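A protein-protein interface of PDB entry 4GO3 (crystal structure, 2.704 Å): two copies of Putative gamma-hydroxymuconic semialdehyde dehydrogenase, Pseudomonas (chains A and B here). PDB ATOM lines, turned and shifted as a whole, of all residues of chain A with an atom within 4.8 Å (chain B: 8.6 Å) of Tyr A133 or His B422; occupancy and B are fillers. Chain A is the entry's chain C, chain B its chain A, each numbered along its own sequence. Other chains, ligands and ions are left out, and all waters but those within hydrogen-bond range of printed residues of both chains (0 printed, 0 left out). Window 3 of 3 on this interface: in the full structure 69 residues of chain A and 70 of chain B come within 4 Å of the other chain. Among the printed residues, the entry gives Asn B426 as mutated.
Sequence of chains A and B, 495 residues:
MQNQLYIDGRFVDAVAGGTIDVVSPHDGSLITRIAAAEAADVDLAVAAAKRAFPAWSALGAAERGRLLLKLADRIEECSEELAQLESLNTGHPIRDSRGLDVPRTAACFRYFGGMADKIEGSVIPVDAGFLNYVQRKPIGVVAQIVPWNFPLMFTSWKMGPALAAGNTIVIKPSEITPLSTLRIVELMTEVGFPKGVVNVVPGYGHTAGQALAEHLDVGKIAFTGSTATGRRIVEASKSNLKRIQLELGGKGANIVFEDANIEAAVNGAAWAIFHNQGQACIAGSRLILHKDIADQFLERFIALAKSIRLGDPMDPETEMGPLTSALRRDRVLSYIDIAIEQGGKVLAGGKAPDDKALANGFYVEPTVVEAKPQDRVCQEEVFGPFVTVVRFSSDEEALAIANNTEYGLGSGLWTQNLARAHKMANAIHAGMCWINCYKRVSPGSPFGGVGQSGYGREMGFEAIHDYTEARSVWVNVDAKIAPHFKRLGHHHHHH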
ATOM      1  N   SER A 122       4.535  22.448  29.862  1.00  0.00           N
ATOM      2  CA  SER A 122       3.876  23.730  29.743  1.00  0.00           C
ATOM      3  C   SER A 122       4.191  24.323  28.395  1.00  0.00           C
ATOM      4  O   SER A 122       5.133  23.909  27.729  1.00  0.00           O
ATOM      5  CB  SER A 122       4.334  24.663  30.866  1.00  0.00           C
ATOM      6  OG  SER A 122       5.634  24.320  31.320  1.00  0.00           O
ATOM      7  N   VAL A 123       3.402  25.317  28.025  1.00  0.00           N
ATOM      8  CA  VAL A 123       3.600  26.051  26.803  1.00  0.00           C
ATOM      9  C   VAL A 123       3.786  27.502  27.147  1.00  0.00           C
ATOM     10  O   VAL A 123       2.966  28.101  27.803  1.00  0.00           O
ATOM     11  CB  VAL A 123       2.423  25.886  25.856  1.00  0.00           C
ATOM     12  CG1 VAL A 123       2.484  26.905  24.772  1.00  0.00           C
ATOM     13  CG2 VAL A 123       2.419  24.515  25.281  1.00  0.00           C
ATOM     14  N   LEU A 131       6.671  28.929  18.770  1.00  0.00           N
ATOM     15  CA  LEU A 131       6.007  28.078  19.708  1.00  0.00           C
ATOM     16  C   LEU A 131       7.062  27.524  20.625  1.00  0.00           C
ATOM     17  O   LEU A 131       7.994  26.886  20.188  1.00  0.00           O
ATOM     18  CB  LEU A 131       5.283  26.964  18.989  1.00  0.00           C
ATOM     19  CG  LEU A 131       4.606  25.949  19.884  1.00  0.00           C
ATOM     20  CD1 LEU A 131       3.295  26.495  20.379  1.00  0.00           C
ATOM     21  CD2 LEU A 131       4.431  24.683  19.101  1.00  0.00           C
ATOM     22  N   ASN A 132       6.908  27.810  21.903  1.00  0.00           N
ATOM     23  CA  ASN A 132       7.758  27.269  22.939  1.00  0.00           C
ATOM     24  C   ASN A 132       6.989  26.299  23.828  1.00  0.00           C
ATOM     25  O   ASN A 132       6.147  26.700  24.585  1.00  0.00           O
ATOM     26  CB  ASN A 132       8.292  28.412  23.778  1.00  0.00           C
ATOM     27  CG  ASN A 132       9.330  27.985  24.739  1.00  0.00           C
ATOM     28  OD1 ASN A 132      10.009  27.003  24.544  1.00  0.00           O
ATOM     29  ND2 ASN A 132       9.486  28.745  25.776  1.00  0.00           N
ATOM     30  N   TYR A 133       7.274  25.016  23.728  1.00  0.00           N
ATOM     31  CA  TYR A 133       6.647  24.061  24.612  1.00  0.00           C
ATOM     32  C   TYR A 133       7.720  23.301  25.367  1.00  0.00           C
ATOM     33  O   TYR A 133       8.711  22.910  24.801  1.00  0.00           O
ATOM     34  CB  TYR A 133       5.711  23.126  23.850  1.00  0.00           C
ATOM     35  CG  TYR A 133       6.410  22.134  22.979  1.00  0.00           C
ATOM     36  CD1 TYR A 133       7.053  21.052  23.524  1.00  0.00           C
ATOM     37  CD2 TYR A 133       6.425  22.280  21.614  1.00  0.00           C
ATOM     38  CE1 TYR A 133       7.684  20.153  22.737  1.00  0.00           C
ATOM     39  CE2 TYR A 133       7.056  21.381  20.827  1.00  0.00           C
ATOM     40  CZ  TYR A 133       7.684  20.319  21.390  1.00  0.00           C
ATOM     41  OH  TYR A 133       8.326  19.410  20.602  1.00  0.00           O
ATOM     42  N   VAL A 134       7.517  23.125  26.660  1.00  0.00           N
ATOM     43  CA  VAL A 134       8.518  22.544  27.529  1.00  0.00           C
ATOM     44  C   VAL A 134       8.004  21.236  28.055  1.00  0.00           C
ATOM     45  O   VAL A 134       7.093  21.212  28.860  1.00  0.00           O
ATOM     46  CB  VAL A 134       8.822  23.457  28.702  1.00  0.00           C
ATOM     47  CG1 VAL A 134       9.879  22.833  29.606  1.00  0.00           C
ATOM     48  CG2 VAL A 134       9.282  24.807  28.172  1.00  0.00           C
ATOM     49  N   GLN A 135       8.603  20.129  27.682  1.00  0.00           N
ATOM     50  CA  GLN A 135       8.242  18.890  28.328  1.00  0.00           C
ATOM     51  C   GLN A 135       8.874  18.745  29.713  1.00  0.00           C
ATOM     52  O   GLN A 135       9.819  19.428  30.050  1.00  0.00           O
ATOM     53  CB  GLN A 135       8.653  17.740  27.458  1.00  0.00           C
ATOM     54  CG  GLN A 135       8.375  17.968  26.037  1.00  0.00           C
ATOM     55  CD  GLN A 135       7.549  16.861  25.461  1.00  0.00           C
ATOM     56  OE1 GLN A 135       7.776  16.423  24.346  1.00  0.00           O
ATOM     57  NE2 GLN A 135       6.585  16.388  26.228  1.00  0.00           N
ATOM     58  N   ARG A 471      12.486  20.100  29.347  1.00  0.00           N
ATOM     59  CA  ARG A 471      13.062  20.025  28.026  1.00  0.00           C
ATOM     60  C   ARG A 471      12.287  20.925  27.086  1.00  0.00           C
ATOM     61  O   ARG A 471      11.330  20.508  26.476  1.00  0.00           O
ATOM     62  CB  ARG A 471      13.076  18.580  27.530  1.00  0.00           C
ATOM     63  CG  ARG A 471      13.818  17.614  28.428  1.00  0.00           C
ATOM     64  CD  ARG A 471      15.148  17.202  27.824  1.00  0.00           C
ATOM     65  NE  ARG A 471      15.245  15.762  27.655  1.00  0.00           N
ATOM     66  CZ  ARG A 471      15.242  15.159  26.481  1.00  0.00           C
ATOM     67  NH1 ARG A 471      15.169  15.876  25.390  1.00  0.00           N
ATOM     68  NH2 ARG A 471      15.318  13.844  26.393  1.00  0.00           N
ATOM     69  N   SER A 472      12.724  22.171  26.989  1.00  0.00           N
ATOM     70  CA  SER A 472      12.052  23.192  26.205  1.00  0.00           C
ATOM     71  C   SER A 472      12.316  23.078  24.741  1.00  0.00           C
ATOM     72  O   SER A 472      13.444  23.084  24.329  1.00  0.00           O
ATOM     73  CB  SER A 472      12.517  24.580  26.625  1.00  0.00           C
ATOM     74  OG  SER A 472      12.158  25.530  25.647  1.00  0.00           O
ATOM     75  N   VAL A 473      11.278  23.006  23.938  1.00  0.00           N
ATOM     76  CA  VAL A 473      11.494  23.006  22.514  1.00  0.00           C
ATOM     77  C   VAL A 473      10.943  24.262  21.878  1.00  0.00           C
ATOM     78  O   VAL A 473       9.846  24.679  22.151  1.00  0.00           O
ATOM     79  CB  VAL A 473      10.943  21.753  21.848  1.00  0.00           C
ATOM     80  CG1 VAL A 473      11.001  21.878  20.363  1.00  0.00           C
ATOM     81  CG2 VAL A 473      11.740  20.577  22.271  1.00  0.00           C
ATOM     82  N   VAL A 475       9.771  26.214  18.349  1.00  0.00           N
ATOM     83  CA  VAL A 475       9.482  26.041  16.938  1.00  0.00           C
ATOM     84  C   VAL A 475       9.333  27.400  16.321  1.00  0.00           C
ATOM     85  O   VAL A 475       8.590  28.215  16.805  1.00  0.00           O
ATOM     86  CB  VAL A 475       8.214  25.230  16.682  1.00  0.00           C
ATOM     87  CG1 VAL A 475       8.079  24.951  15.222  1.00  0.00           C
ATOM     88  CG2 VAL A 475       8.237  23.939  17.472  1.00  0.00           C
ATOM     89  N   PHE B 257      19.070  19.813   7.947  1.00  0.00           N
ATOM     90  CA  PHE B 257      18.552  18.769   7.103  1.00  0.00           C
ATOM     91  C   PHE B 257      18.363  19.222   5.679  1.00  0.00           C
ATOM     92  O   PHE B 257      18.315  20.395   5.402  1.00  0.00           O
ATOM     93  CB  PHE B 257      17.237  18.278   7.663  1.00  0.00           C
ATOM     94  CG  PHE B 257      17.376  17.494   8.912  1.00  0.00           C
ATOM     95  CD1 PHE B 257      17.799  16.194   8.880  1.00  0.00           C
ATOM     96  CD2 PHE B 257      17.076  18.058  10.123  1.00  0.00           C
ATOM     97  CE1 PHE B 257      17.922  15.486  10.023  1.00  0.00           C
ATOM     98  CE2 PHE B 257      17.198  17.346  11.273  1.00  0.00           C
ATOM     99  CZ  PHE B 257      17.614  16.065  11.225  1.00  0.00           C
ATOM    100  N   LEU B 413      17.834  22.466  15.144  1.00  0.00           N
ATOM    101  CA  LEU B 413      17.818  21.793  13.871  1.00  0.00           C
ATOM    102  C   LEU B 413      16.999  22.603  12.877  1.00  0.00           C
ATOM    103  O   LEU B 413      16.263  23.512  13.248  1.00  0.00           O
ATOM    104  CB  LEU B 413      17.265  20.388  14.046  1.00  0.00           C
ATOM    105  CG  LEU B 413      15.897  20.372  14.718  1.00  0.00           C
ATOM    106  CD1 LEU B 413      14.858  20.469  13.646  1.00  0.00           C
ATOM    107  CD2 LEU B 413      15.719  19.098  15.489  1.00  0.00           C
ATOM    108  N   THR B 415      14.539  22.176   9.488  1.00  0.00           N
ATOM    109  CA  THR B 415      13.696  21.501   8.519  1.00  0.00           C
ATOM    110  C   THR B 415      12.377  22.165   8.319  1.00  0.00           C
ATOM    111  O   THR B 415      11.922  22.965   9.102  1.00  0.00           O
ATOM    112  CB  THR B 415      13.197  20.167   8.977  1.00  0.00           C
ATOM    113  OG1 THR B 415      13.630  19.925  10.290  1.00  0.00           O
ATOM    114  CG2 THR B 415      13.648  19.101   8.084  1.00  0.00           C
ATOM    115  N   ASN B 417      10.057  19.540   7.699  1.00  0.00           N
ATOM    116  CA  ASN B 417       9.306  18.336   7.958  1.00  0.00           C
ATOM    117  C   ASN B 417       8.771  18.309   9.375  1.00  0.00           C
ATOM    118  O   ASN B 417       9.542  18.342  10.336  1.00  0.00           O
ATOM    119  CB  ASN B 417      10.176  17.103   7.737  1.00  0.00           C
ATOM    120  CG  ASN B 417       9.376  15.829   7.794  1.00  0.00           C
ATOM    121  OD1 ASN B 417       8.558  15.585   6.926  1.00  0.00           O
ATOM    122  ND2 ASN B 417       9.598  15.024   8.825  1.00  0.00           N
ATOM    123  N   LEU B 418       7.453  18.216   9.496  1.00  0.00           N
ATOM    124  CA  LEU B 418       6.787  18.226  10.791  1.00  0.00           C
ATOM    125  C   LEU B 418       7.278  17.113  11.713  1.00  0.00           C
ATOM    126  O   LEU B 418       7.801  17.372  12.796  1.00  0.00           O
ATOM    127  CB  LEU B 418       5.283  18.112  10.572  1.00  0.00           C
ATOM    128  CG  LEU B 418       4.447  17.904  11.816  1.00  0.00           C
ATOM    129  CD1 LEU B 418       4.553  19.154  12.669  1.00  0.00           C
ATOM    130  CD2 LEU B 418       3.007  17.611  11.379  1.00  0.00           C
ATOM    131  N   ALA B 419       7.128  15.910  11.252  1.00  0.00           N
ATOM    132  CA  ALA B 419       7.533  14.815  12.021  1.00  0.00           C
ATOM    133  C   ALA B 419       8.935  15.092  12.488  1.00  0.00           C
ATOM    134  O   ALA B 419       9.150  15.314  13.638  1.00  0.00           O
ATOM    135  CB  ALA B 419       7.454  13.589  11.195  1.00  0.00           C
ATOM    136  N   ARG B 420       9.875  15.101  11.561  1.00  0.00           N
ATOM    137  CA  ARG B 420      11.289  15.178  11.805  1.00  0.00           C
ATOM    138  C   ARG B 420      11.632  16.127  12.858  1.00  0.00           C
ATOM    139  O   ARG B 420      12.369  15.815  13.755  1.00  0.00           O
ATOM    140  CB  ARG B 420      11.969  15.642  10.570  1.00  0.00           C
ATOM    141  CG  ARG B 420      13.420  15.700  10.738  1.00  0.00           C
ATOM    142  CD  ARG B 420      14.065  16.198   9.540  1.00  0.00           C
ATOM    143  NE  ARG B 420      14.312  15.116   8.620  1.00  0.00           N
ATOM    144  CZ  ARG B 420      14.385  15.252   7.320  1.00  0.00           C
ATOM    145  NH1 ARG B 420      14.248  16.406   6.772  1.00  0.00           N
ATOM    146  NH2 ARG B 420      14.591  14.217   6.585  1.00  0.00           N
ATOM    147  N   ALA B 421      11.111  17.314  12.726  1.00  0.00           N
ATOM    148  CA  ALA B 421      11.292  18.381  13.704  1.00  0.00           C
ATOM    149  C   ALA B 421      11.040  17.897  15.137  1.00  0.00           C
ATOM    150  O   ALA B 421      11.905  18.043  15.999  1.00  0.00           O
ATOM    151  CB  ALA B 421      10.401  19.563  13.376  1.00  0.00           C
ATOM    152  N   HIS B 422       9.873  17.312  15.392  1.00  0.00           N
ATOM    153  CA  HIS B 422       9.529  16.912  16.748  1.00  0.00           C
ATOM    154  C   HIS B 422      10.241  15.645  17.174  1.00  0.00           C
ATOM    155  O   HIS B 422      10.721  15.559  18.304  1.00  0.00           O
ATOM    156  CB  HIS B 422       8.023  16.783  16.909  1.00  0.00           C
ATOM    157  CG  HIS B 422       7.304  18.075  16.722  1.00  0.00           C
ATOM    158  ND1 HIS B 422       7.428  19.127  17.606  1.00  0.00           N
ATOM    159  CD2 HIS B 422       6.473  18.502  15.742  1.00  0.00           C
ATOM    160  CE1 HIS B 422       6.695  20.144  17.182  1.00  0.00           C
ATOM    161  NE2 HIS B 422       6.109  19.791  16.050  1.00  0.00           N
ATOM    162  N   LYS B 423      10.383  14.716  16.264  1.00  0.00           N
ATOM    163  CA  LYS B 423      11.044  13.512  16.597  1.00  0.00           C
ATOM    164  C   LYS B 423      12.399  13.785  17.099  1.00  0.00           C
ATOM    165  O   LYS B 423      12.808  13.253  18.079  1.00  0.00           O
ATOM    166  CB  LYS B 423      11.138  12.638  15.416  1.00  0.00           C
ATOM    167  CG  LYS B 423      11.674  11.352  15.836  1.00  0.00           C
ATOM    168  CD  LYS B 423      11.036  10.208  15.166  1.00  0.00           C
ATOM    169  CE  LYS B 423      12.038   9.353  14.449  1.00  0.00           C
ATOM    170  NZ  LYS B 423      11.610   9.160  13.047  1.00  0.00           N
ATOM    171  N   MET B 424      13.088  14.679  16.416  1.00  0.00           N
ATOM    172  CA  MET B 424      14.451  15.000  16.757  1.00  0.00           C
ATOM    173  C   MET B 424      14.560  15.826  18.020  1.00  0.00           C
ATOM    174  O   MET B 424      15.368  15.532  18.865  1.00  0.00           O
ATOM    175  CB  MET B 424      15.120  15.690  15.584  1.00  0.00           C
ATOM    176  CG  MET B 424      15.181  14.833  14.356  1.00  0.00           C
ATOM    177  SD  MET B 424      16.625  13.789  14.339  1.00  0.00           S
ATOM    178  CE  MET B 424      17.859  14.973  14.785  1.00  0.00           C
ATOM    179  N   ALA B 425      13.735  16.847  18.158  1.00  0.00           N
ATOM    180  CA  ALA B 425      13.684  17.630  19.384  1.00  0.00           C
ATOM    181  C   ALA B 425      13.419  16.760  20.628  1.00  0.00           C
ATOM    182  O   ALA B 425      14.017  16.981  21.667  1.00  0.00           O
ATOM    183  CB  ALA B 425      12.648  18.699  19.261  1.00  0.00           C
ATOM    184  N   ASN B 426      12.578  15.757  20.468  1.00  0.00           N
ATOM    185  CA  ASN B 426      12.170  14.867  21.521  1.00  0.00           C
ATOM    186  C   ASN B 426      13.251  13.848  21.822  1.00  0.00           C
ATOM    187  O   ASN B 426      13.293  13.285  22.897  1.00  0.00           O
ATOM    188  CB  ASN B 426      10.854  14.219  21.087  1.00  0.00           C
ATOM    189  CG  ASN B 426      10.505  12.988  21.858  1.00  0.00           C
ATOM    190  OD1 ASN B 426      10.094  13.057  23.000  1.00  0.00           O
ATOM    191  ND2 ASN B 426      10.621  11.846  21.216  1.00  0.00           N
ATOM    192  N   ALA B 427      14.149  13.643  20.877  1.00  0.00           N
ATOM    193  CA  ALA B 427      15.180  12.625  20.985  1.00  0.00           C
ATOM    194  C   ALA B 427      16.553  13.178  21.337  1.00  0.00           C
ATOM    195  O   ALA B 427      17.434  12.413  21.733  1.00  0.00           O
ATOM    196  CB  ALA B 427      15.250  11.808  19.704  1.00  0.00           C
ATOM    197  N   ILE B 428      16.742  14.484  21.222  1.00  0.00           N
ATOM    198  CA  ILE B 428      18.020  15.078  21.572  1.00  0.00           C
ATOM    199  C   ILE B 428      18.102  15.311  23.064  1.00  0.00           C
ATOM    200  O   ILE B 428      17.278  15.998  23.616  1.00  0.00           O
ATOM    201  CB  ILE B 428      18.236  16.432  20.901  1.00  0.00           C
ATOM    202  CG1 ILE B 428      17.958  16.362  19.415  1.00  0.00           C
ATOM    203  CG2 ILE B 428      19.651  16.854  21.061  1.00  0.00           C
ATOM    204  CD1 ILE B 428      18.603  17.460  18.630  1.00  0.00           C
ATOM    205  N   GLY B 431      18.602  20.328  27.257  1.00  0.00           N
ATOM    206  CA  GLY B 431      17.588  21.025  28.028  1.00  0.00           C
ATOM    207  C   GLY B 431      16.688  21.855  27.126  1.00  0.00           C
ATOM    208  O   GLY B 431      15.504  22.037  27.393  1.00  0.00           O
ATOM    209  N   MET B 432      17.267  22.388  26.060  1.00  0.00           N
ATOM    210  CA  MET B 432      16.545  23.223  25.108  1.00  0.00           C
ATOM    211  C   MET B 432      16.822  22.801  23.680  1.00  0.00           C
ATOM    212  O   MET B 432      17.903  22.362  23.377  1.00  0.00           O
ATOM    213  CB  MET B 432      16.963  24.678  25.256  1.00  0.00           C
ATOM    214  CG  MET B 432      16.907  25.184  26.649  1.00  0.00           C
ATOM    215  SD  MET B 432      18.200  26.338  26.981  1.00  0.00           S
ATOM    216  CE  MET B 432      19.533  25.238  27.299  1.00  0.00           C
ATOM    217  N   CYS B 433      15.841  22.950  22.802  1.00  0.00           N
ATOM    218  CA  CYS B 433      16.038  22.632  21.405  1.00  0.00           C
ATOM    219  C   CYS B 433      15.296  23.623  20.545  1.00  0.00           C
ATOM    220  O   CYS B 433      14.082  23.803  20.704  1.00  0.00           O
ATOM    221  CB  CYS B 433      15.512  21.232  21.108  1.00  0.00           C
ATOM    222  SG  CYS B 433      15.776  20.728  19.390  1.00  0.00           S
ATOM    223  N   ILE B 435      14.084  24.897  16.743  1.00  0.00           N
ATOM    224  CA  ILE B 435      13.781  24.423  15.397  1.00  0.00           C
ATOM    225  C   ILE B 435      13.574  25.597  14.434  1.00  0.00           C
ATOM    226  O   ILE B 435      12.706  26.450  14.633  1.00  0.00           O
ATOM    227  CB  ILE B 435      12.566  23.509  15.407  1.00  0.00           C
ATOM    228  CG1 ILE B 435      12.815  22.337  16.356  1.00  0.00           C
ATOM    229  CG2 ILE B 435      12.273  23.004  13.990  1.00  0.00           C
ATOM    230  CD1 ILE B 435      11.541  21.551  16.734  1.00  0.00           C
ATOM    231  N   SER B 445      10.807  31.081  29.525  1.00  0.00           N
ATOM    232  CA  SER B 445      11.138  29.772  28.971  1.00  0.00           C
ATOM    233  C   SER B 445      12.340  29.175  29.680  1.00  0.00           C
ATOM    234  O   SER B 445      13.449  29.653  29.499  1.00  0.00           O
ATOM    235  CB  SER B 445      11.429  29.889  27.478  1.00  0.00           C
ATOM    236  OG  SER B 445      11.751  28.639  26.901  1.00  0.00           O
ATOM    237  N   PRO B 446      12.124  28.107  30.464  1.00  0.00           N
ATOM    238  CA  PRO B 446      13.164  27.495  31.296  1.00  0.00           C
ATOM    239  C   PRO B 446      14.434  27.240  30.512  1.00  0.00           C
ATOM    240  O   PRO B 446      14.394  26.690  29.416  1.00  0.00           O
ATOM    241  CB  PRO B 446      12.551  26.161  31.699  1.00  0.00           C
ATOM    242  CG  PRO B 446      11.122  26.378  31.602  1.00  0.00           C
ATOM    243  CD  PRO B 446      10.909  27.289  30.440  1.00  0.00           C
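No position is printed for both chains.
The side-chain amide oxygen of Asn A132 sits close to the backbone carbonyl oxygen of Val A473 (3.3 Å). N of Val A134 lies within hydrogen-bond range of O of Ser A122 (2.7 Å). The backbone carbonyl oxygen (O) of Gln A135 is in hydrogen-bond range of the backbone NH (N) of Arg A471. The backbone NH (N) of Val A473 lies within hydrogen-bond range of the backbone carbonyl oxygen (O) of Tyr A133, 2.7 Å away. O of Leu A131 sits at hydrogen-bond distance from N of Val A475, at 2.6 Å. The side-chain amide oxygen (OD1) of Asn A132 lies within hydrogen-bond range of the side-chain hydroxyl (OG) of Ser A472.
Of the 21 printed residues of chain B, 9 touch a printed residue of chain A. Printed residues of chain B that touch a printed residue of chain A: His B422, Ala B425, Ile B428, Gly B431, Met B432, Cys B433, Ile B435, Ser B445 and Pro B446. Hydrophobic or aromatic side chains of chain B that line the printed part of chain A: His B422, Ala B425, Met B432, Ile B435 and Pro B446. Of the 11 printed residues of chain A, 7 touch a printed residue of chain B. Printed residues of chain A that touch a printed residue of chain B: Asn A132, Tyr A133, Val A134, Arg A471, Ser A472, Val A473 and Val A475. Hydrophobic or aromatic side chains of chain A within 4 Å of the printed part of chain B: Tyr A133, Val A134 and Val A473. Among the printed residues, 14 pairs touch across the chains. Among the printed residues, no Asp or Glu carboxylate lies within 4 Å of a Lys or Arg side-chain nitrogen of the other chain.
NH1 of Arg A471 lies within hydrogen-bond range of O of Ile B428 (2.8 Å). A ring nitrogen (ND1) of His B422 lies within hydrogen-bond range of the side-chain hydroxyl of Tyr A133 (3.1 Å). OG of Ser A472 is in hydrogen-bond range of OG of Ser B445 (3.4 Å). The backbone carbonyl oxygen (O) of Ser A472 lies within hydrogen-bond range of the backbone NH (N) of Cys B433 (2.8 Å). The backbone carbonyl oxygen (O) of Gly B431 sits at hydrogen-bond distance from the backbone NH (N) of Ser A472 (2.8 Å). OG of Ser B445 lies within hydrogen-bond range of ND2 of Asn A132, 2.5 Å away.
Among the printed residues, pairs that only touch across the chains: Ser A472 with Met B432 (3.2 Å), Arg A471 with Gly B431 (3.2 Å), Val A473 with Cys B433 (3.3 Å), Val A473 with Ala B425 (3.7 Å), Val A473 with Ile B435 (3.7 Å), Val A134 with Pro B446 (3.7 Å), Val A475 with Ile B435 (3.9 Å) and Ser A472 with Pro B446 (3.97 Å).
Tyr A133 touches just one residue of chain B: His B422 (3.1 Å). Of the printed residues of chain A, His B422 touches Tyr A133 (3.1 Å). Val A473 touches just these residues of chain B: Ala B425 (3.7 Å), Cys B433 (3.3 Å) and Ile B435 (3.7 Å). Of the printed residues of chain A, Met B432 touches Ser A472 (3.2 Å). Printed residues of chain A within 4 Å of Ile B435: Val A473 and Val A475. The nearest residue of chain B that does not touch Tyr A133 is Ala B425 (4.6 Å).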
